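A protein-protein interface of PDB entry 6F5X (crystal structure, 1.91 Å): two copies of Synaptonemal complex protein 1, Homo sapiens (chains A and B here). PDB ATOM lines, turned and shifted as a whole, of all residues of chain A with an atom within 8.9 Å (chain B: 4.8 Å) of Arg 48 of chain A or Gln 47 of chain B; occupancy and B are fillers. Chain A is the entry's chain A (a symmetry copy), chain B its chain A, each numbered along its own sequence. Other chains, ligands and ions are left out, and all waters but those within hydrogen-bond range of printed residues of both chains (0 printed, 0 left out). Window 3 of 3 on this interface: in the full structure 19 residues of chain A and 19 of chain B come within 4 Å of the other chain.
Lys 42 of chain A touches none of the printed residues of chain B.
Of the printed residues of chain B, Ile 43 of chain A touches Ile 44 (3.99 Å).
Printed residues of chain B within 4 Å of Gln 47 of chain A: Ile 44, Gln 47 and Arg 48.
Printed residues of chain A within 4 Å of Ile 43 of chain B: Ile 44 (3.99 Å).
Printed residues of chain A within 4 Å of Ile 44 of chain B: Asn 40, Ile 43, Ile 44 and Gln 47.
Ala 46 of chain B touches none of the printed residues of chain A.
Of the printed residues of chain A, Gln 47 of chain B touches Ile 44 (3.4 Å), Gln 47 (2.6 Å) and Arg 48 (3.2 Å).
Of the printed residues of chain A, Arg 48 of chain B touches Gln 47 (3.2 Å).
The nearest printed residue of chain B that does not touch Arg 48 of chain A is Ile 51 of chain B (5.9 Å).
NE2 of Gln 47 of chain A lies within hydrogen-bond range of O of Ile 44 of chain B, 3.4 Å away.
NE2 of Gln 47 of chain B is in hydrogen-bond range of O of Ile 44 of chain A, at 3.4 Å.
OE1 of Gln 47 of chain B sits close to OE1 of Gln 47 of chain A, 2.6 Å away.
The backbone NH (N) of Arg 48 of chain A sits close to the side-chain amide nitrogen (NE2) of Gln 47 of chain B (3.2 Å).
The backbone NH of Arg 48 of chain B lies close to the side-chain amide nitrogen of Gln 47 of chain A (3.2 Å).
Printed residues of chain A that touch a printed residue of chain B: Asn 40, Ile 43, Ile 44, Gln 47, Arg 48 and Ile 51.
Hydrophobic or aromatic side chains of chain A within 4 Å of the printed part of chain B: Ile 43, Ile 44 and Ile 51.
Of the 9 printed residues of chain B, 5 touch a printed residue of chain A.
Among the printed residues, no Asp or Glu carboxylate lies within 4 Å of a Lys or Arg side-chain nitrogen of the other chain.
Ile 44 of chain B touches Asn 40 of chain A (CD1 to OD1, 3.5 Å).
CG2 of Ile 44 of chain B touches CG2 of Ile 43 of chain A, at 3.99 Å.
Ile 43 of chain B touches Ile 44 of chain A.
Ile 44 of chain A touches Ile 44 of chain B (CG1 to CG1, 3.5 Å).
Ile 51 of chain B touches Ile 51 of chain A.
Ile 43 of chain A touches Ile 44 of chain B, and with the chains exchanged Ile 44 of chain A touches Ile 43 of chain B.
Gln 47 of chain A touches its own counterpart, Gln 47 of chain B.
Gln 47 of chain A touches Arg 48 of chain B, and with the chains exchanged Arg 48 of chain A touches Gln 47 of chain B.
Ile 51 of chain B touches its own counterpart, Ile 51 of chain A.
Positions printed for both chains: 43, 44, 45, 46, 47, 48, 49, 50 and 51.
Of the 10 pairs that touch across the chains among the printed residues, 9 have their exchanged pair printed and touching as well.
The side-chain carboxylate (OE2) of Glu 45 of chain B lies within salt-bridge range of the guanidinium group (NH2) of Arg 48 of chain B, 2.4 Å away.
The guanidinium group (NH2) of Arg 48 of chain A lies within salt-bridge range of the side-chain carboxylate (OE2) of Glu 45 of chain A (2.4 Å).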
ATOM      1  N   ASN A  40      -0.767 -20.849   5.635  1.00  0.00           N
ATOM      2  CA  ASN A  40      -1.445 -19.655   5.140  1.00  0.00           C
ATOM      3  C   ASN A  40      -2.808 -19.483   5.790  1.00  0.00           C
ATOM      4  O   ASN A  40      -3.190 -18.365   6.148  1.00  0.00           O
ATOM      5  CB  ASN A  40      -1.612 -19.694   3.624  1.00  0.00           C
ATOM      6  CG  ASN A  40      -0.312 -19.529   2.886  1.00  0.00           C
ATOM      7  OD1 ASN A  40       0.577 -18.803   3.322  1.00  0.00           O
ATOM      8  ND2 ASN A  40      -0.231 -20.124   1.708  1.00  0.00           N
ATOM      9  N   ARG A  41      -3.574 -20.571   5.919  1.00  0.00           N
ATOM     10  CA  ARG A  41      -4.868 -20.451   6.578  1.00  0.00           C
ATOM     11  C   ARG A  41      -4.705 -19.933   7.999  1.00  0.00           C
ATOM     12  O   ARG A  41      -5.476 -19.070   8.444  1.00  0.00           O
ATOM     13  CB  ARG A  41      -5.620 -21.780   6.563  1.00  0.00           C
ATOM     14  CG  ARG A  41      -6.341 -22.080   5.256  1.00  0.00           C
ATOM     15  CD  ARG A  41      -5.458 -22.808   4.261  1.00  0.00           C
ATOM     16  NE  ARG A  41      -6.208 -23.322   3.115  1.00  0.00           N
ATOM     17  CZ  ARG A  41      -6.345 -22.680   1.960  1.00  0.00           C
ATOM     18  NH1 ARG A  41      -5.776 -21.494   1.789  1.00  0.00           N
ATOM     19  NH2 ARG A  41      -7.049 -23.222   0.976  1.00  0.00           N
ATOM     20  N   LYS A  42      -3.684 -20.415   8.715  1.00  0.00           N
ATOM     21  CA  LYS A  42      -3.454 -19.899  10.064  1.00  0.00           C
ATOM     22  C   LYS A  42      -3.193 -18.392  10.047  1.00  0.00           C
ATOM     23  O   LYS A  42      -3.821 -17.630  10.796  1.00  0.00           O
ATOM     24  CB  LYS A  42      -2.293 -20.639  10.725  1.00  0.00           C
ATOM     25  CG  LYS A  42      -2.482 -22.149  10.851  1.00  0.00           C
ATOM     26  CD  LYS A  42      -3.634 -22.516  11.777  1.00  0.00           C
ATOM     27  CE  LYS A  42      -3.675 -24.018  12.047  1.00  0.00           C
ATOM     28  NZ  LYS A  42      -4.052 -24.835  10.851  1.00  0.00           N
ATOM     29  N   ILE A  43      -2.264 -17.941   9.201  1.00  0.00           N
ATOM     30  CA  ILE A  43      -1.941 -16.515   9.156  1.00  0.00           C
ATOM     31  C   ILE A  43      -3.176 -15.692   8.814  1.00  0.00           C
ATOM     32  O   ILE A  43      -3.440 -14.654   9.434  1.00  0.00           O
ATOM     33  CB  ILE A  43      -0.801 -16.260   8.156  1.00  0.00           C
ATOM     34  CG1 ILE A  43       0.486 -16.943   8.617  1.00  0.00           C
ATOM     35  CG2 ILE A  43      -0.569 -14.788   7.961  1.00  0.00           C
ATOM     36  CD1 ILE A  43       1.572 -16.958   7.549  1.00  0.00           C
ATOM     37  N   ILE A  44      -3.964 -16.150   7.838  1.00  0.00           N
ATOM     38  CA  ILE A  44      -5.112 -15.371   7.376  1.00  0.00           C
ATOM     39  C   ILE A  44      -6.166 -15.249   8.470  1.00  0.00           C
ATOM     40  O   ILE A  44      -6.714 -14.162   8.704  1.00  0.00           O
ATOM     41  CB  ILE A  44      -5.687 -15.989   6.087  1.00  0.00           C
ATOM     42  CG1 ILE A  44      -4.664 -15.868   4.955  1.00  0.00           C
ATOM     43  CG2 ILE A  44      -7.003 -15.335   5.699  1.00  0.00           C
ATOM     44  CD1 ILE A  44      -5.014 -16.635   3.715  1.00  0.00           C
ATOM     45  N   GLU A  45      -6.479 -16.353   9.151  1.00  0.00           N
ATOM     46  CA  GLU A  45      -7.438 -16.284  10.251  1.00  0.00           C
ATOM     47  C   GLU A  45      -6.931 -15.379  11.366  1.00  0.00           C
ATOM     48  O   GLU A  45      -7.691 -14.566  11.919  1.00  0.00           O
ATOM     49  CB  GLU A  45      -7.716 -17.694  10.773  1.00  0.00           C
ATOM     50  CG  GLU A  45      -8.734 -17.783  11.897  1.00  0.00           C
ATOM     51  CD  GLU A  45     -10.133 -17.397  11.467  1.00  0.00           C
ATOM     52  OE1 GLU A  45     -10.433 -17.498  10.259  1.00  0.00           O
ATOM     53  OE2 GLU A  45     -10.940 -17.023  12.344  1.00  0.00           O
ATOM     54  N   ALA A  46      -5.640 -15.491  11.695  1.00  0.00           N
ATOM     55  CA  ALA A  46      -5.018 -14.592  12.668  1.00  0.00           C
ATOM     56  C   ALA A  46      -5.238 -13.121  12.308  1.00  0.00           C
ATOM     57  O   ALA A  46      -5.719 -12.323  13.128  1.00  0.00           O
ATOM     58  CB  ALA A  46      -3.520 -14.903  12.769  1.00  0.00           C
ATOM     59  N   GLN A  47      -4.883 -12.739  11.082  1.00  0.00           N
ATOM     60  CA  GLN A  47      -4.997 -11.340  10.669  1.00  0.00           C
ATOM     61  C   GLN A  47      -6.449 -10.881  10.642  1.00  0.00           C
ATOM     62  O   GLN A  47      -6.751  -9.728  10.975  1.00  0.00           O
ATOM     63  CB  GLN A  47      -4.371 -11.140   9.288  1.00  0.00           C
ATOM     64  CG  GLN A  47      -2.863 -11.332   9.200  1.00  0.00           C
ATOM     65  CD  GLN A  47      -2.347 -11.073   7.793  1.00  0.00           C
ATOM     66  OE1 GLN A  47      -2.809 -11.686   6.838  1.00  0.00           O
ATOM     67  NE2 GLN A  47      -1.396 -10.156   7.662  1.00  0.00           N
ATOM     68  N   ARG A  48      -7.356 -11.761  10.210  1.00  0.00           N
ATOM     69  CA  ARG A  48      -8.779 -11.446  10.239  1.00  0.00           C
ATOM     70  C   ARG A  48      -9.226 -11.078  11.649  1.00  0.00           C
ATOM     71  O   ARG A  48      -9.814 -10.010  11.872  1.00  0.00           O
ATOM     72  CB  ARG A  48      -9.594 -12.637   9.747  1.00  0.00           C
ATOM     73  CG  ARG A  48     -11.082 -12.317   9.673  1.00  0.00           C
ATOM     74  CD  ARG A  48     -11.936 -13.541   9.381  1.00  0.00           C
ATOM     75  NE  ARG A  48     -11.926 -14.482  10.503  1.00  0.00           N
ATOM     76  CZ  ARG A  48     -12.715 -14.389  11.575  1.00  0.00           C
ATOM     77  NH1 ARG A  48     -13.596 -13.401  11.684  1.00  0.00           N
ATOM     78  NH2 ARG A  48     -12.634 -15.294  12.542  1.00  0.00           N
ATOM     79  N   LYS A  49      -8.970 -11.964  12.619  1.00  0.00           N
ATOM     80  CA  LYS A  49      -9.384 -11.656  13.984  1.00  0.00           C
ATOM     81  C   LYS A  49      -8.722 -10.381  14.490  1.00  0.00           C
ATOM     82  O   LYS A  49      -9.361  -9.584  15.187  1.00  0.00           O
ATOM     83  CB  LYS A  49      -9.103 -12.829  14.923  1.00  0.00           C
ATOM     84  CG  LYS A  49      -9.990 -14.052  14.680  1.00  0.00           C
ATOM     85  CD  LYS A  49     -11.460 -13.731  14.968  1.00  0.00           C
ATOM     86  CE  LYS A  49     -11.732 -13.536  16.454  1.00  0.00           C
ATOM     87  NZ  LYS A  49     -13.178 -13.288  16.721  1.00  0.00           N
ATOM     88  N   ALA A  50      -7.456 -10.152  14.118  1.00  0.00           N
ATOM     89  CA  ALA A  50      -6.767  -8.931  14.529  1.00  0.00           C
ATOM     90  C   ALA A  50      -7.484  -7.683  14.014  1.00  0.00           C
ATOM     91  O   ALA A  50      -7.781  -6.754  14.781  1.00  0.00           O
ATOM     92  CB  ALA A  50      -5.323  -8.965  14.038  1.00  0.00           C
ATOM     93  N   ILE A  51      -7.753  -7.636  12.707  1.00  0.00           N
ATOM     94  CA  ILE A  51      -8.494  -6.518  12.122  1.00  0.00           C
ATOM     95  C   ILE A  51      -9.846  -6.339  12.818  1.00  0.00           C
ATOM     96  O   ILE A  51     -10.279  -5.207  13.092  1.00  0.00           O
ATOM     97  CB  ILE A  51      -8.649  -6.737  10.601  1.00  0.00           C
ATOM     98  CG1 ILE A  51      -7.279  -6.723   9.921  1.00  0.00           C
ATOM     99  CG2 ILE A  51      -9.515  -5.666   9.989  1.00  0.00           C
ATOM    100  CD1 ILE A  51      -7.293  -7.203   8.482  1.00  0.00           C
ATOM    101  N   GLN A  52     -10.530  -7.451  13.121  1.00  0.00           N
ATOM    102  CA  GLN A  52     -11.812  -7.380  13.829  1.00  0.00           C
ATOM    103  C   GLN A  52     -11.661  -6.676  15.175  1.00  0.00           C
ATOM    104  O   GLN A  52     -12.446  -5.783  15.523  1.00  0.00           O
ATOM    105  CB  GLN A  52     -12.390  -8.796  14.033  1.00  0.00           C
ATOM    106  CG  GLN A  52     -13.796  -8.838  14.699  1.00  0.00           C
ATOM    107  CD  GLN A  52     -14.356 -10.261  14.927  1.00  0.00           C
ATOM    108  OE1 GLN A  52     -13.684 -11.262  14.666  1.00  0.00           O
ATOM    109  NE2 GLN A  52     -15.602 -10.343  15.392  1.00  0.00           N
ATOM    110  N   GLU A  53     -10.669  -7.096  15.966  1.00  0.00           N
ATOM    111  CA  GLU A  53     -10.455  -6.497  17.278  1.00  0.00           C
ATOM    112  C   GLU A  53     -10.083  -5.024  17.174  1.00  0.00           C
ATOM    113  O   GLU A  53     -10.529  -4.207  17.986  1.00  0.00           O
ATOM    114  CB  GLU A  53      -9.357  -7.253  18.017  1.00  0.00           C
ATOM    115  CG  GLU A  53      -9.722  -8.665  18.416  1.00  0.00           C
ATOM    116  CD  GLU A  53      -8.559  -9.375  19.082  1.00  0.00           C
ATOM    117  OE1 GLU A  53      -7.447  -8.801  19.083  1.00  0.00           O
ATOM    118  OE2 GLU A  53      -8.752 -10.498  19.602  1.00  0.00           O
ATOM    119  N   LEU A  54      -9.218  -4.676  16.217  1.00  0.00           N
ATOM    120  CA  LEU A  54      -8.833  -3.277  16.023  1.00  0.00           C
ATOM    121  C   LEU A  54     -10.033  -2.398  15.678  1.00  0.00           C
ATOM    122  O   LEU A  54     -10.177  -1.281  16.206  1.00  0.00           O
ATOM    123  CB  LEU A  54      -7.762  -3.180  14.926  1.00  0.00           C
ATOM    124  CG  LEU A  54      -6.357  -3.702  15.234  1.00  0.00           C
ATOM    125  CD1 LEU A  54      -5.515  -3.744  13.965  1.00  0.00           C
ATOM    126  CD2 LEU A  54      -5.690  -2.803  16.260  1.00  0.00           C
ATOM    127  N   GLN A  55     -10.902  -2.872  14.790  1.00  0.00           N
ATOM    128  CA  GLN A  55     -12.061  -2.068  14.409  1.00  0.00           C
ATOM    129  C   GLN A  55     -13.059  -1.945  15.560  1.00  0.00           C
ATOM    130  O   GLN A  55     -13.641  -0.871  15.779  1.00  0.00           O
ATOM    131  CB  GLN A  55     -12.700  -2.679  13.165  1.00  0.00           C
ATOM    132  CG  GLN A  55     -11.821  -2.497  11.922  1.00  0.00           C
ATOM    133  CD  GLN A  55     -12.354  -3.214  10.696  1.00  0.00           C
ATOM    134  OE1 GLN A  55     -13.308  -3.994  10.771  1.00  0.00           O
ATOM    135  NE2 GLN A  55     -11.759  -2.924   9.547  1.00  0.00           N
ATOM    136  N   ILE B  43      -4.129 -12.174  -0.259  1.00  0.00           N
ATOM    137  CA  ILE B  43      -4.919 -11.867   0.934  1.00  0.00           C
ATOM    138  C   ILE B  43      -4.014 -11.462   2.090  1.00  0.00           C
ATOM    139  O   ILE B  43      -4.291 -10.489   2.803  1.00  0.00           O
ATOM    140  CB  ILE B  43      -5.804 -13.068   1.307  1.00  0.00           C
ATOM    141  CG1 ILE B  43      -6.833 -13.342   0.212  1.00  0.00           C
ATOM    142  CG2 ILE B  43      -6.492 -12.846   2.625  1.00  0.00           C
ATOM    143  CD1 ILE B  43      -7.558 -14.671   0.389  1.00  0.00           C
ATOM    144  N   ILE B  44      -2.908 -12.185   2.284  1.00  0.00           N
ATOM    145  CA  ILE B  44      -2.039 -11.929   3.431  1.00  0.00           C
ATOM    146  C   ILE B  44      -1.388 -10.555   3.329  1.00  0.00           C
ATOM    147  O   ILE B  44      -1.335  -9.804   4.313  1.00  0.00           O
ATOM    148  CB  ILE B  44      -0.995 -13.055   3.565  1.00  0.00           C
ATOM    149  CG1 ILE B  44      -1.695 -14.372   3.904  1.00  0.00           C
ATOM    150  CG2 ILE B  44       0.054 -12.715   4.612  1.00  0.00           C
ATOM    151  CD1 ILE B  44      -0.813 -15.583   3.834  1.00  0.00           C
ATOM    152  N   GLU B  45      -0.872 -10.204   2.149  1.00  0.00           N
ATOM    153  CA  GLU B  45      -0.289  -8.875   1.975  1.00  0.00           C
ATOM    154  C   GLU B  45      -1.333  -7.786   2.181  1.00  0.00           C
ATOM    155  O   GLU B  45      -1.066  -6.768   2.842  1.00  0.00           O
ATOM    156  CB  GLU B  45       0.341  -8.774   0.586  1.00  0.00           C
ATOM    157  CG  GLU B  45       1.028  -7.454   0.277  1.00  0.00           C
ATOM    158  CD  GLU B  45       2.257  -7.209   1.126  1.00  0.00           C
ATOM    159  OE1 GLU B  45       2.849  -8.194   1.614  1.00  0.00           O
ATOM    160  OE2 GLU B  45       2.646  -6.032   1.277  1.00  0.00           O
ATOM    161  N   ALA B  46      -2.538  -7.993   1.641  1.00  0.00           N
ATOM    162  CA  ALA B  46      -3.651  -7.072   1.875  1.00  0.00           C
ATOM    163  C   ALA B  46      -3.891  -6.833   3.367  1.00  0.00           C
ATOM    164  O   ALA B  46      -3.933  -5.685   3.837  1.00  0.00           O
ATOM    165  CB  ALA B  46      -4.918  -7.616   1.207  1.00  0.00           C
ATOM    166  N   GLN B  47      -4.058  -7.911   4.132  1.00  0.00           N
ATOM    167  CA  GLN B  47      -4.355  -7.781   5.558  1.00  0.00           C
ATOM    168  C   GLN B  47      -3.200  -7.139   6.315  1.00  0.00           C
ATOM    169  O   GLN B  47      -3.416  -6.367   7.258  1.00  0.00           O
ATOM    170  CB  GLN B  47      -4.667  -9.150   6.165  1.00  0.00           C
ATOM    171  CG  GLN B  47      -5.941  -9.826   5.678  1.00  0.00           C
ATOM    172  CD  GLN B  47      -6.168 -11.160   6.372  1.00  0.00           C
ATOM    173  OE1 GLN B  47      -5.306 -12.031   6.344  1.00  0.00           O
ATOM    174  NE2 GLN B  47      -7.323 -11.317   7.007  1.00  0.00           N
ATOM    175  N   ARG B  48      -1.965  -7.479   5.939  1.00  0.00           N
ATOM    176  CA  ARG B  48      -0.797  -6.845   6.539  1.00  0.00           C
ATOM    177  C   ARG B  48      -0.857  -5.331   6.376  1.00  0.00           C
ATOM    178  O   ARG B  48      -0.759  -4.581   7.358  1.00  0.00           O
ATOM    179  CB  ARG B  48       0.480  -7.371   5.893  1.00  0.00           C
ATOM    180  CG  ARG B  48       1.729  -6.803   6.556  1.00  0.00           C
ATOM    181  CD  ARG B  48       3.006  -7.150   5.806  1.00  0.00           C
ATOM    182  NE  ARG B  48       3.067  -6.474   4.509  1.00  0.00           N
ATOM    183  CZ  ARG B  48       3.494  -5.222   4.328  1.00  0.00           C
ATOM    184  NH1 ARG B  48       3.913  -4.494   5.356  1.00  0.00           N
ATOM    185  NH2 ARG B  48       3.515  -4.696   3.110  1.00  0.00           N
ATOM    186  N   LYS B  49      -1.002  -4.857   5.132  1.00  0.00           N
ATOM    187  CA  LYS B  49      -1.060  -3.413   4.929  1.00  0.00           C
ATOM    188  C   LYS B  49      -2.232  -2.795   5.678  1.00  0.00           C
ATOM    189  O   LYS B  49      -2.102  -1.698   6.236  1.00  0.00           O
ATOM    190  CB  LYS B  49      -1.118  -3.070   3.440  1.00  0.00           C
ATOM    191  CG  LYS B  49       0.177  -3.361   2.679  1.00  0.00           C
ATOM    192  CD  LYS B  49       1.324  -2.482   3.187  1.00  0.00           C
ATOM    193  CE  LYS B  49       1.150  -1.019   2.799  1.00  0.00           C
ATOM    194  NZ  LYS B  49       2.307  -0.190   3.246  1.00  0.00           N
ATOM    195  N   ALA B  50      -3.370  -3.497   5.736  1.00  0.00           N
ATOM    196  CA  ALA B  50      -4.524  -2.987   6.472  1.00  0.00           C
ATOM    197  C   ALA B  50      -4.199  -2.781   7.951  1.00  0.00           C
ATOM    198  O   ALA B  50      -4.443  -1.702   8.514  1.00  0.00           O
ATOM    199  CB  ALA B  50      -5.702  -3.944   6.307  1.00  0.00           C
ATOM    200  N   ILE B  51      -3.665  -3.816   8.603  1.00  0.00           N
ATOM    201  CA  ILE B  51      -3.255  -3.704  10.004  1.00  0.00           C
ATOM    202  C   ILE B  51      -2.260  -2.554  10.189  1.00  0.00           C
ATOM    203  O   ILE B  51      -2.336  -1.794  11.168  1.00  0.00           O
ATOM    204  CB  ILE B  51      -2.677  -5.052  10.485  1.00  0.00           C
ATOM    205  CG1 ILE B  51      -3.761  -6.132  10.459  1.00  0.00           C
ATOM    206  CG2 ILE B  51      -2.132  -4.935  11.885  1.00  0.00           C
ATOM    207  CD1 ILE B  51      -3.237  -7.544  10.644  1.00  0.00           C
